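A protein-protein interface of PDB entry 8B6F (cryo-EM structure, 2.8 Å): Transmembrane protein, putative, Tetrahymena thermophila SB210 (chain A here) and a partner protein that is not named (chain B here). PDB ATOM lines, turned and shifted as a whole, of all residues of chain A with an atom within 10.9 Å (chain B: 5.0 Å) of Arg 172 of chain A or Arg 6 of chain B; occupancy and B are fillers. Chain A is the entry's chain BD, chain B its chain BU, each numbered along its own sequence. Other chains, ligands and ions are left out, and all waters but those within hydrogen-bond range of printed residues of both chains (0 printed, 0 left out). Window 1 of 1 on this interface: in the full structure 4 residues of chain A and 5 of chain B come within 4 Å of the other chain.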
ATOM      1  N   LEU A 160      -4.775  26.395 -19.047  1.00  0.00           N
ATOM      2  CA  LEU A 160      -3.934  25.242 -18.748  1.00  0.00           C
ATOM      3  C   LEU A 160      -2.813  25.576 -17.774  1.00  0.00           C
ATOM      4  O   LEU A 160      -2.223  24.659 -17.195  1.00  0.00           O
ATOM      5  CB  LEU A 160      -3.343  24.662 -20.033  1.00  0.00           C
ATOM      6  CG  LEU A 160      -4.290  23.878 -20.944  1.00  0.00           C
ATOM      7  CD1 LEU A 160      -3.554  23.410 -22.186  1.00  0.00           C
ATOM      8  CD2 LEU A 160      -4.903  22.691 -20.221  1.00  0.00           C
ATOM      9  N   ALA A 163      -3.448  23.757 -14.968  1.00  0.00           N
ATOM     10  CA  ALA A 163      -3.589  22.320 -15.204  1.00  0.00           C
ATOM     11  C   ALA A 163      -2.240  21.768 -15.647  1.00  0.00           C
ATOM     12  O   ALA A 163      -2.037  21.455 -16.826  1.00  0.00           O
ATOM     13  CB  ALA A 163      -4.668  22.036 -16.248  1.00  0.00           C
ATOM     14  N   PRO A 164      -1.288  21.641 -14.720  1.00  0.00           N
ATOM     15  CA  PRO A 164       0.072  21.250 -15.127  1.00  0.00           C
ATOM     16  C   PRO A 164       0.138  19.932 -15.877  1.00  0.00           C
ATOM     17  O   PRO A 164       0.910  19.816 -16.835  1.00  0.00           O
ATOM     18  CB  PRO A 164       0.826  21.182 -13.791  1.00  0.00           C
ATOM     19  CG  PRO A 164       0.055  22.052 -12.872  1.00  0.00           C
ATOM     20  CD  PRO A 164      -1.375  21.903 -13.274  1.00  0.00           C
ATOM     21  N   ILE A 165      -0.641  18.928 -15.471  1.00  0.00           N
ATOM     22  CA  ILE A 165      -0.581  17.636 -16.150  1.00  0.00           C
ATOM     23  C   ILE A 165      -1.079  17.768 -17.583  1.00  0.00           C
ATOM     24  O   ILE A 165      -0.407  17.350 -18.532  1.00  0.00           O
ATOM     25  CB  ILE A 165      -1.383  16.577 -15.373  1.00  0.00           C
ATOM     26  CG1 ILE A 165      -0.799  16.399 -13.971  1.00  0.00           C
ATOM     27  CG2 ILE A 165      -1.386  15.251 -16.129  1.00  0.00           C
ATOM     28  CD1 ILE A 165      -1.561  15.423 -13.106  1.00  0.00           C
ATOM     29  N   THR A 166      -2.261  18.356 -17.762  1.00  0.00           N
ATOM     30  CA  THR A 166      -2.816  18.488 -19.104  1.00  0.00           C
ATOM     31  C   THR A 166      -1.954  19.403 -19.962  1.00  0.00           C
ATOM     32  O   THR A 166      -1.817  19.184 -21.170  1.00  0.00           O
ATOM     33  CB  THR A 166      -4.246  19.011 -19.030  1.00  0.00           C
ATOM     34  OG1 THR A 166      -5.005  18.196 -18.130  1.00  0.00           O
ATOM     35  CG2 THR A 166      -4.896  18.972 -20.403  1.00  0.00           C
ATOM     36  N   ARG A 167      -1.374  20.439 -19.356  1.00  0.00           N
ATOM     37  CA  ARG A 167      -0.511  21.345 -20.104  1.00  0.00           C
ATOM     38  C   ARG A 167       0.667  20.591 -20.708  1.00  0.00           C
ATOM     39  O   ARG A 167       0.932  20.692 -21.912  1.00  0.00           O
ATOM     40  CB  ARG A 167      -0.026  22.461 -19.181  1.00  0.00           C
ATOM     41  CG  ARG A 167       0.945  23.443 -19.813  1.00  0.00           C
ATOM     42  CD  ARG A 167       1.404  24.458 -18.783  1.00  0.00           C
ATOM     43  NE  ARG A 167       2.043  23.806 -17.646  1.00  0.00           N
ATOM     44  CZ  ARG A 167       2.229  24.368 -16.461  1.00  0.00           C
ATOM     45  NH1 ARG A 167       1.828  25.602 -16.209  1.00  0.00           N
ATOM     46  NH2 ARG A 167       2.829  23.671 -15.501  1.00  0.00           N
ATOM     47  N   ARG A 168       1.392  19.834 -19.885  1.00  0.00           N
ATOM     48  CA  ARG A 168       2.550  19.103 -20.386  1.00  0.00           C
ATOM     49  C   ARG A 168       2.137  18.030 -21.384  1.00  0.00           C
ATOM     50  O   ARG A 168       2.785  17.857 -22.423  1.00  0.00           O
ATOM     51  CB  ARG A 168       3.320  18.491 -19.218  1.00  0.00           C
ATOM     52  CG  ARG A 168       3.862  19.526 -18.243  1.00  0.00           C
ATOM     53  CD  ARG A 168       4.366  18.891 -16.959  1.00  0.00           C
ATOM     54  NE  ARG A 168       5.502  18.006 -17.185  1.00  0.00           N
ATOM     55  CZ  ARG A 168       6.153  17.363 -16.225  1.00  0.00           C
ATOM     56  NH1 ARG A 168       5.810  17.486 -14.953  1.00  0.00           N
ATOM     57  NH2 ARG A 168       7.172  16.573 -16.549  1.00  0.00           N
ATOM     58  N   ALA A 169       1.062  17.296 -21.089  1.00  0.00           N
ATOM     59  CA  ALA A 169       0.603  16.255 -22.003  1.00  0.00           C
ATOM     60  C   ALA A 169       0.197  16.845 -23.347  1.00  0.00           C
ATOM     61  O   ALA A 169       0.505  16.280 -24.403  1.00  0.00           O
ATOM     62  CB  ALA A 169      -0.563  15.488 -21.382  1.00  0.00           C
ATOM     63  N   TRP A 170      -0.500  17.983 -23.323  1.00  0.00           N
ATOM     64  CA  TRP A 170      -0.923  18.632 -24.560  1.00  0.00           C
ATOM     65  C   TRP A 170       0.271  19.153 -25.351  1.00  0.00           C
ATOM     66  O   TRP A 170       0.293  19.058 -26.583  1.00  0.00           O
ATOM     67  CB  TRP A 170      -1.901  19.762 -24.232  1.00  0.00           C
ATOM     68  CG  TRP A 170      -2.411  20.511 -25.422  1.00  0.00           C
ATOM     69  CD1 TRP A 170      -2.135  21.804 -25.748  1.00  0.00           C
ATOM     70  CD2 TRP A 170      -3.286  20.016 -26.442  1.00  0.00           C
ATOM     71  NE1 TRP A 170      -2.785  22.146 -26.908  1.00  0.00           N
ATOM     72  CE2 TRP A 170      -3.498  21.065 -27.353  1.00  0.00           C
ATOM     73  CE3 TRP A 170      -3.912  18.787 -26.671  1.00  0.00           C
ATOM     74  CZ2 TRP A 170      -4.309  20.925 -28.478  1.00  0.00           C
ATOM     75  CZ3 TRP A 170      -4.717  18.648 -27.787  1.00  0.00           C
ATOM     76  CH2 TRP A 170      -4.908  19.711 -28.677  1.00  0.00           C
ATOM     77  N   GLU A 171       1.274  19.701 -24.664  1.00  0.00           N
ATOM     78  CA  GLU A 171       2.480  20.147 -25.355  1.00  0.00           C
ATOM     79  C   GLU A 171       3.168  18.980 -26.053  1.00  0.00           C
ATOM     80  O   GLU A 171       3.574  19.087 -27.217  1.00  0.00           O
ATOM     81  CB  GLU A 171       3.429  20.819 -24.365  1.00  0.00           C
ATOM     82  CG  GLU A 171       4.711  21.341 -24.995  1.00  0.00           C
ATOM     83  CD  GLU A 171       5.642  21.974 -23.980  1.00  0.00           C
ATOM     84  OE1 GLU A 171       5.269  22.033 -22.789  1.00  0.00           O
ATOM     85  OE2 GLU A 171       6.744  22.409 -24.372  1.00  0.00           O
ATOM     86  N   ARG A 172       3.322  17.857 -25.350  1.00  0.00           N
ATOM     87  CA  ARG A 172       3.950  16.688 -25.957  1.00  0.00           C
ATOM     88  C   ARG A 172       3.134  16.179 -27.137  1.00  0.00           C
ATOM     89  O   ARG A 172       3.691  15.839 -28.186  1.00  0.00           O
ATOM     90  CB  ARG A 172       4.125  15.584 -24.917  1.00  0.00           C
ATOM     91  CG  ARG A 172       5.094  15.927 -23.801  1.00  0.00           C
ATOM     92  CD  ARG A 172       5.071  14.859 -22.724  1.00  0.00           C
ATOM     93  NE  ARG A 172       5.405  13.545 -23.258  1.00  0.00           N
ATOM     94  CZ  ARG A 172       5.227  12.403 -22.609  1.00  0.00           C
ATOM     95  NH1 ARG A 172       4.700  12.372 -21.396  1.00  0.00           N
ATOM     96  NH2 ARG A 172       5.583  11.263 -23.193  1.00  0.00           N
ATOM     97  N   ALA A 173       1.810  16.128 -26.987  1.00  0.00           N
ATOM     98  CA  ALA A 173       0.960  15.647 -28.070  1.00  0.00           C
ATOM     99  C   ALA A 173       1.050  16.556 -29.287  1.00  0.00           C
ATOM    100  O   ALA A 173       1.097  16.079 -30.426  1.00  0.00           O
ATOM    101  CB  ALA A 173      -0.487  15.533 -27.592  1.00  0.00           C
ATOM    102  N   LEU A 174       1.067  17.872 -29.071  1.00  0.00           N
ATOM    103  CA  LEU A 174       1.212  18.797 -30.190  1.00  0.00           C
ATOM    104  C   LEU A 174       2.552  18.617 -30.893  1.00  0.00           C
ATOM    105  O   LEU A 174       2.620  18.643 -32.126  1.00  0.00           O
ATOM    106  CB  LEU A 174       1.056  20.240 -29.715  1.00  0.00           C
ATOM    107  CG  LEU A 174      -0.352  20.724 -29.361  1.00  0.00           C
ATOM    108  CD1 LEU A 174      -0.289  22.169 -28.912  1.00  0.00           C
ATOM    109  CD2 LEU A 174      -1.315  20.571 -30.528  1.00  0.00           C
ATOM    110  N   ALA A 175       3.629  18.432 -30.128  1.00  0.00           N
ATOM    111  CA  ALA A 175       4.933  18.217 -30.745  1.00  0.00           C
ATOM    112  C   ALA A 175       4.932  16.957 -31.601  1.00  0.00           C
ATOM    113  O   ALA A 175       5.422  16.961 -32.735  1.00  0.00           O
ATOM    114  CB  ALA A 175       6.011  18.133 -29.665  1.00  0.00           C
ATOM    115  N   THR A 176       4.377  15.865 -31.076  1.00  0.00           N
ATOM    116  CA  THR A 176       4.342  14.617 -31.829  1.00  0.00           C
ATOM    117  C   THR A 176       3.485  14.754 -33.078  1.00  0.00           C
ATOM    118  O   THR A 176       3.841  14.241 -34.145  1.00  0.00           O
ATOM    119  CB  THR A 176       3.820  13.488 -30.948  1.00  0.00           C
ATOM    120  OG1 THR A 176       2.493  13.804 -30.513  1.00  0.00           O
ATOM    121  CG2 THR A 176       4.720  13.289 -29.756  1.00  0.00           C
ATOM    122  N   ASN A 177       2.348  15.438 -32.962  1.00  0.00           N
ATOM    123  CA  ASN A 177       1.497  15.652 -34.125  1.00  0.00           C
ATOM    124  C   ASN A 177       2.217  16.483 -35.177  1.00  0.00           C
ATOM    125  O   ASN A 177       2.109  16.208 -36.377  1.00  0.00           O
ATOM    126  CB  ASN A 177       0.199  16.334 -33.702  1.00  0.00           C
ATOM    127  CG  ASN A 177      -0.666  16.721 -34.883  1.00  0.00           C
ATOM    128  OD1 ASN A 177      -1.281  17.787 -34.891  1.00  0.00           O
ATOM    129  ND2 ASN A 177      -0.731  15.850 -35.883  1.00  0.00           N
ATOM    130  N   GLN A 178       2.958  17.506 -34.747  1.00  0.00           N
ATOM    131  CA  GLN A 178       3.709  18.314 -35.699  1.00  0.00           C
ATOM    132  C   GLN A 178       4.762  17.476 -36.411  1.00  0.00           C
ATOM    133  O   GLN A 178       4.953  17.605 -37.625  1.00  0.00           O
ATOM    134  CB  GLN A 178       4.357  19.498 -34.981  1.00  0.00           C
ATOM    135  CG  GLN A 178       4.971  20.530 -35.911  1.00  0.00           C
ATOM    136  CD  GLN A 178       3.936  21.250 -36.747  1.00  0.00           C
ATOM    137  OE1 GLN A 178       2.733  21.086 -36.547  1.00  0.00           O
ATOM    138  NE2 GLN A 178       4.399  22.055 -37.698  1.00  0.00           N
ATOM    139  N   GLU A 179       5.463  16.614 -35.671  1.00  0.00           N
ATOM    140  CA  GLU A 179       6.438  15.731 -36.304  1.00  0.00           C
ATOM    141  C   GLU A 179       5.759  14.792 -37.291  1.00  0.00           C
ATOM    142  O   GLU A 179       6.279  14.546 -38.385  1.00  0.00           O
ATOM    143  CB  GLU A 179       7.202  14.933 -35.246  1.00  0.00           C
ATOM    144  CG  GLU A 179       8.441  15.635 -34.702  1.00  0.00           C
ATOM    145  CD  GLU A 179       8.179  16.381 -33.408  1.00  0.00           C
ATOM    146  OE1 GLU A 179       7.638  15.765 -32.466  1.00  0.00           O
ATOM    147  OE2 GLU A 179       8.515  17.582 -33.330  1.00  0.00           O
ATOM    148  N   TYR A 180       4.597  14.255 -36.917  1.00  0.00           N
ATOM    149  CA  TYR A 180       3.864  13.366 -37.812  1.00  0.00           C
ATOM    150  C   TYR A 180       3.457  14.085 -39.092  1.00  0.00           C
ATOM    151  O   TYR A 180       3.595  13.538 -40.192  1.00  0.00           O
ATOM    152  CB  TYR A 180       2.637  12.815 -37.087  1.00  0.00           C
ATOM    153  CG  TYR A 180       1.767  11.896 -37.911  1.00  0.00           C
ATOM    154  CD1 TYR A 180       2.124  10.568 -38.118  1.00  0.00           C
ATOM    155  CD2 TYR A 180       0.569  12.344 -38.450  1.00  0.00           C
ATOM    156  CE1 TYR A 180       1.322   9.720 -38.856  1.00  0.00           C
ATOM    157  CE2 TYR A 180      -0.240  11.504 -39.191  1.00  0.00           C
ATOM    158  CZ  TYR A 180       0.142  10.193 -39.389  1.00  0.00           C
ATOM    159  OH  TYR A 180      -0.661   9.355 -40.128  1.00  0.00           O
ATOM    160  N   GLN A 181       2.949  15.313 -38.969  1.00  0.00           N
ATOM    161  CA  GLN A 181       2.567  16.081 -40.149  1.00  0.00           C
ATOM    162  C   GLN A 181       3.775  16.392 -41.023  1.00  0.00           C
ATOM    163  O   GLN A 181       3.693  16.327 -42.253  1.00  0.00           O
ATOM    164  CB  GLN A 181       1.858  17.367 -39.731  1.00  0.00           C
ATOM    165  CG  GLN A 181       0.485  17.132 -39.129  1.00  0.00           C
ATOM    166  CD  GLN A 181      -0.212  18.420 -38.756  1.00  0.00           C
ATOM    167  OE1 GLN A 181       0.388  19.494 -38.775  1.00  0.00           O
ATOM    168  NE2 GLN A 181      -1.493  18.321 -38.420  1.00  0.00           N
ATOM    169  N   ALA B   1      11.078  11.625 -32.333  1.00  0.00           N
ATOM    170  CA  ALA B   1      12.121  12.633 -31.989  1.00  0.00           C
ATOM    171  C   ALA B   1      12.006  13.049 -30.529  1.00  0.00           C
ATOM    172  O   ALA B   1      12.909  12.806 -29.730  1.00  0.00           O
ATOM    173  CB  ALA B   1      12.005  13.846 -32.894  1.00  0.00           C
ATOM    174  N   SER B   2      10.885  13.685 -30.187  1.00  0.00           N
ATOM    175  CA  SER B   2      10.687  14.148 -28.818  1.00  0.00           C
ATOM    176  C   SER B   2      10.660  12.978 -27.843  1.00  0.00           C
ATOM    177  O   SER B   2      11.310  13.014 -26.793  1.00  0.00           O
ATOM    178  CB  SER B   2       9.396  14.960 -28.726  1.00  0.00           C
ATOM    179  OG  SER B   2       8.287  14.199 -29.174  1.00  0.00           O
ATOM    180  N   GLN B   3       9.909  11.925 -28.177  1.00  0.00           N
ATOM    181  CA  GLN B   3       9.832  10.769 -27.289  1.00  0.00           C
ATOM    182  C   GLN B   3      11.185  10.080 -27.166  1.00  0.00           C
ATOM    183  O   GLN B   3      11.578   9.659 -26.073  1.00  0.00           O
ATOM    184  CB  GLN B   3       8.774   9.791 -27.800  1.00  0.00           C
ATOM    185  CG  GLN B   3       8.421   8.682 -26.822  1.00  0.00           C
ATOM    186  CD  GLN B   3       7.682   9.189 -25.602  1.00  0.00           C
ATOM    187  OE1 GLN B   3       7.458  10.389 -25.451  1.00  0.00           O
ATOM    188  NE2 GLN B   3       7.294   8.272 -24.723  1.00  0.00           N
ATOM    189  N   LEU B   4      11.914   9.955 -28.279  1.00  0.00           N
ATOM    190  CA  LEU B   4      13.235   9.338 -28.228  1.00  0.00           C
ATOM    191  C   LEU B   4      14.180  10.143 -27.347  1.00  0.00           C
ATOM    192  O   LEU B   4      14.920   9.574 -26.536  1.00  0.00           O
ATOM    193  CB  LEU B   4      13.797   9.197 -29.645  1.00  0.00           C
ATOM    194  CG  LEU B   4      15.010   8.281 -29.868  1.00  0.00           C
ATOM    195  CD1 LEU B   4      15.181   8.003 -31.350  1.00  0.00           C
ATOM    196  CD2 LEU B   4      16.307   8.857 -29.307  1.00  0.00           C
ATOM    197  N   GLN B   5      14.156  11.470 -27.474  1.00  0.00           N
ATOM    198  CA  GLN B   5      15.012  12.305 -26.641  1.00  0.00           C
ATOM    199  C   GLN B   5      14.625  12.190 -25.174  1.00  0.00           C
ATOM    200  O   GLN B   5      15.492  12.165 -24.294  1.00  0.00           O
ATOM    201  CB  GLN B   5      14.941  13.759 -27.107  1.00  0.00           C
ATOM    202  CG  GLN B   5      15.909  14.683 -26.389  1.00  0.00           C
ATOM    203  CD  GLN B   5      15.917  16.079 -26.979  1.00  0.00           C
ATOM    204  OE1 GLN B   5      15.229  16.355 -27.961  1.00  0.00           O
ATOM    205  NE2 GLN B   5      16.700  16.970 -26.381  1.00  0.00           N
ATOM    206  N   ARG B   6      13.323  12.125 -24.889  1.00  0.00           N
ATOM    207  CA  ARG B   6      12.871  11.964 -23.513  1.00  0.00           C
ATOM    208  C   ARG B   6      13.376  10.651 -22.924  1.00  0.00           C
ATOM    209  O   ARG B   6      13.860  10.611 -21.788  1.00  0.00           O
ATOM    210  CB  ARG B   6      11.345  12.026 -23.468  1.00  0.00           C
ATOM    211  CG  ARG B   6      10.750  12.088 -22.076  1.00  0.00           C
ATOM    212  CD  ARG B   6       9.232  12.086 -22.150  1.00  0.00           C
ATOM    213  NE  ARG B   6       8.614  12.215 -20.837  1.00  0.00           N
ATOM    214  CZ  ARG B   6       8.323  13.370 -20.251  1.00  0.00           C
ATOM    215  NH1 ARG B   6       8.593  14.528 -20.830  1.00  0.00           N
ATOM    216  NH2 ARG B   6       7.747  13.360 -19.053  1.00  0.00           N
ATOM    217  N   GLU B   7      13.269   9.562 -23.688  1.00  0.00           N
ATOM    218  CA  GLU B   7      13.745   8.269 -23.206  1.00  0.00           C
ATOM    219  C   GLU B   7      15.258   8.271 -23.014  1.00  0.00           C
ATOM    220  O   GLU B   7      15.765   7.711 -22.037  1.00  0.00           O
ATOM    221  CB  GLU B   7      13.328   7.161 -24.171  1.00  0.00           C
ATOM    222  CG  GLU B   7      11.825   6.948 -24.238  1.00  0.00           C
ATOM    223  CD  GLU B   7      11.434   5.858 -25.214  1.00  0.00           C
ATOM    224  OE1 GLU B   7      12.336   5.161 -25.723  1.00  0.00           O
ATOM    225  OE2 GLU B   7      10.223   5.698 -25.473  1.00  0.00           O
ATOM    226  N   GLN B   8      15.993   8.897 -23.936  1.00  0.00           N
ATOM    227  CA  GLN B   8      17.444   8.979 -23.797  1.00  0.00           C
ATOM    228  C   GLN B   8      17.830   9.775 -22.559  1.00  0.00           C
ATOM    229  O   GLN B   8      18.767   9.408 -21.841  1.00  0.00           O
ATOM    230  CB  GLN B   8      18.059   9.600 -25.052  1.00  0.00           C
ATOM    231  CG  GLN B   8      19.581   9.567 -25.074  1.00  0.00           C
ATOM    232  CD  GLN B   8      20.154  10.066 -26.388  1.00  0.00           C
ATOM    233  OE1 GLN B   8      19.416  10.441 -27.298  1.00  0.00           O
ATOM    234  NE2 GLN B   8      21.479  10.074 -26.490  1.00  0.00           N
ATOM    235  N   LYS B   9      17.115  10.869 -22.288  1.00  0.00           N
ATOM    236  CA  LYS B   9      17.369  11.637 -21.075  1.00  0.00           C
ATOM    237  C   LYS B   9      17.097  10.800 -19.833  1.00  0.00           C
ATOM    238  O   LYS B   9      17.848  10.868 -18.853  1.00  0.00           O
ATOM    239  CB  LYS B   9      16.515  12.905 -21.076  1.00  0.00           C
ATOM    240  CG  LYS B   9      16.571  13.700 -19.777  1.00  0.00           C
ATOM    241  CD  LYS B   9      15.884  15.054 -19.916  1.00  0.00           C
ATOM    242  CE  LYS B   9      14.418  14.924 -20.319  1.00  0.00           C
ATOM    243  NZ  LYS B   9      13.639  14.056 -19.389  1.00  0.00           N
ATOM    244  N   LEU B  10      16.025  10.007 -19.849  1.00  0.00           N
ATOM    245  CA  LEU B  10      15.750   9.122 -18.721  1.00  0.00           C
ATOM    246  C   LEU B  10      16.881   8.122 -18.520  1.00  0.00           C
ATOM    247  O   LEU B  10      17.297   7.864 -17.385  1.00  0.00           O
ATOM    248  CB  LEU B  10      14.430   8.384 -18.941  1.00  0.00           C
ATOM    249  CG  LEU B  10      14.077   7.338 -17.878  1.00  0.00           C
ATOM    250  CD1 LEU B  10      13.937   7.992 -16.513  1.00  0.00           C
ATOM    251  CD2 LEU B  10      12.816   6.583 -18.256  1.00  0.00           C
ATOM    252  N   ILE B 133       7.910  10.026 -15.390  1.00  0.00           N
ATOM    253  CA  ILE B 133       9.011  10.979 -15.465  1.00  0.00           C
ATOM    254  C   ILE B 133       8.482  12.342 -15.045  1.00  0.00           C
ATOM    255  O   ILE B 133       7.417  12.767 -15.506  1.00  0.00           O
ATOM    256  CB  ILE B 133       9.613  11.052 -16.880  1.00  0.00           C
ATOM    257  CG1 ILE B 133      10.070   9.665 -17.338  1.00  0.00           C
ATOM    258  CG2 ILE B 133      10.780  12.038 -16.908  1.00  0.00           C
ATOM    259  CD1 ILE B 133      10.594   9.634 -18.765  1.00  0.00           C
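The guanidinium group of Arg 172 of chain A lies within hydrogen-bond range of the side-chain amide oxygen of Gln 3 of chain B (3.1 Å).
O of Ala 175 of chain A lies close to OE1 of Glu 179 of chain A, 2.5 Å away. O of Arg 172 of chain A lies close to OG1 of Thr 176 of chain A (3.3 Å). The side-chain hydroxyl of Thr 176 of chain A sits at hydrogen-bond distance from the backbone carbonyl oxygen of Ala 173 of chain A, 2.7 Å away.
Ile 133 of chain B touches Arg 168 of chain A (O to NH2, 3.95 Å). Arg 6 of chain B touches Arg 172 of chain A (NE to CZ, 3.8 Å). Thr 176 of chain A touches Ser 2 of chain B (CG2 to OG, 3.7 Å). Glu 179 of chain A touches Ser 2 of chain B.
Arg 6 of chain B touches just one residue of chain A: Arg 172. Ser 2 of chain B touches just these residues of chain A: Thr 176 and Glu 179. No residue of chain A comes within 4 Å of Gln 5 of chain B. No residue of chain A comes within 4 Å of Glu 7 of chain B. No residue of chain A comes within 4 Å of Lys 9 of chain B. No residue of chain A comes within 4 Å of Leu 10 of chain B. Ile 133 of chain B touches just one residue of chain A: Arg 168. Of the printed residues of chain B, Thr 176 of chain A touches Ser 2. Printed residues of chain B within 4 Å of Arg 168 of chain A: Ile 133. Tyr 180 of chain A touches none of the printed residues of chain B. The nearest residue of chain A that does not touch Arg 6 of chain B is Arg 168 of chain A (4.1 Å).
Among the printed residues, 5 pairs touch across the chains.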
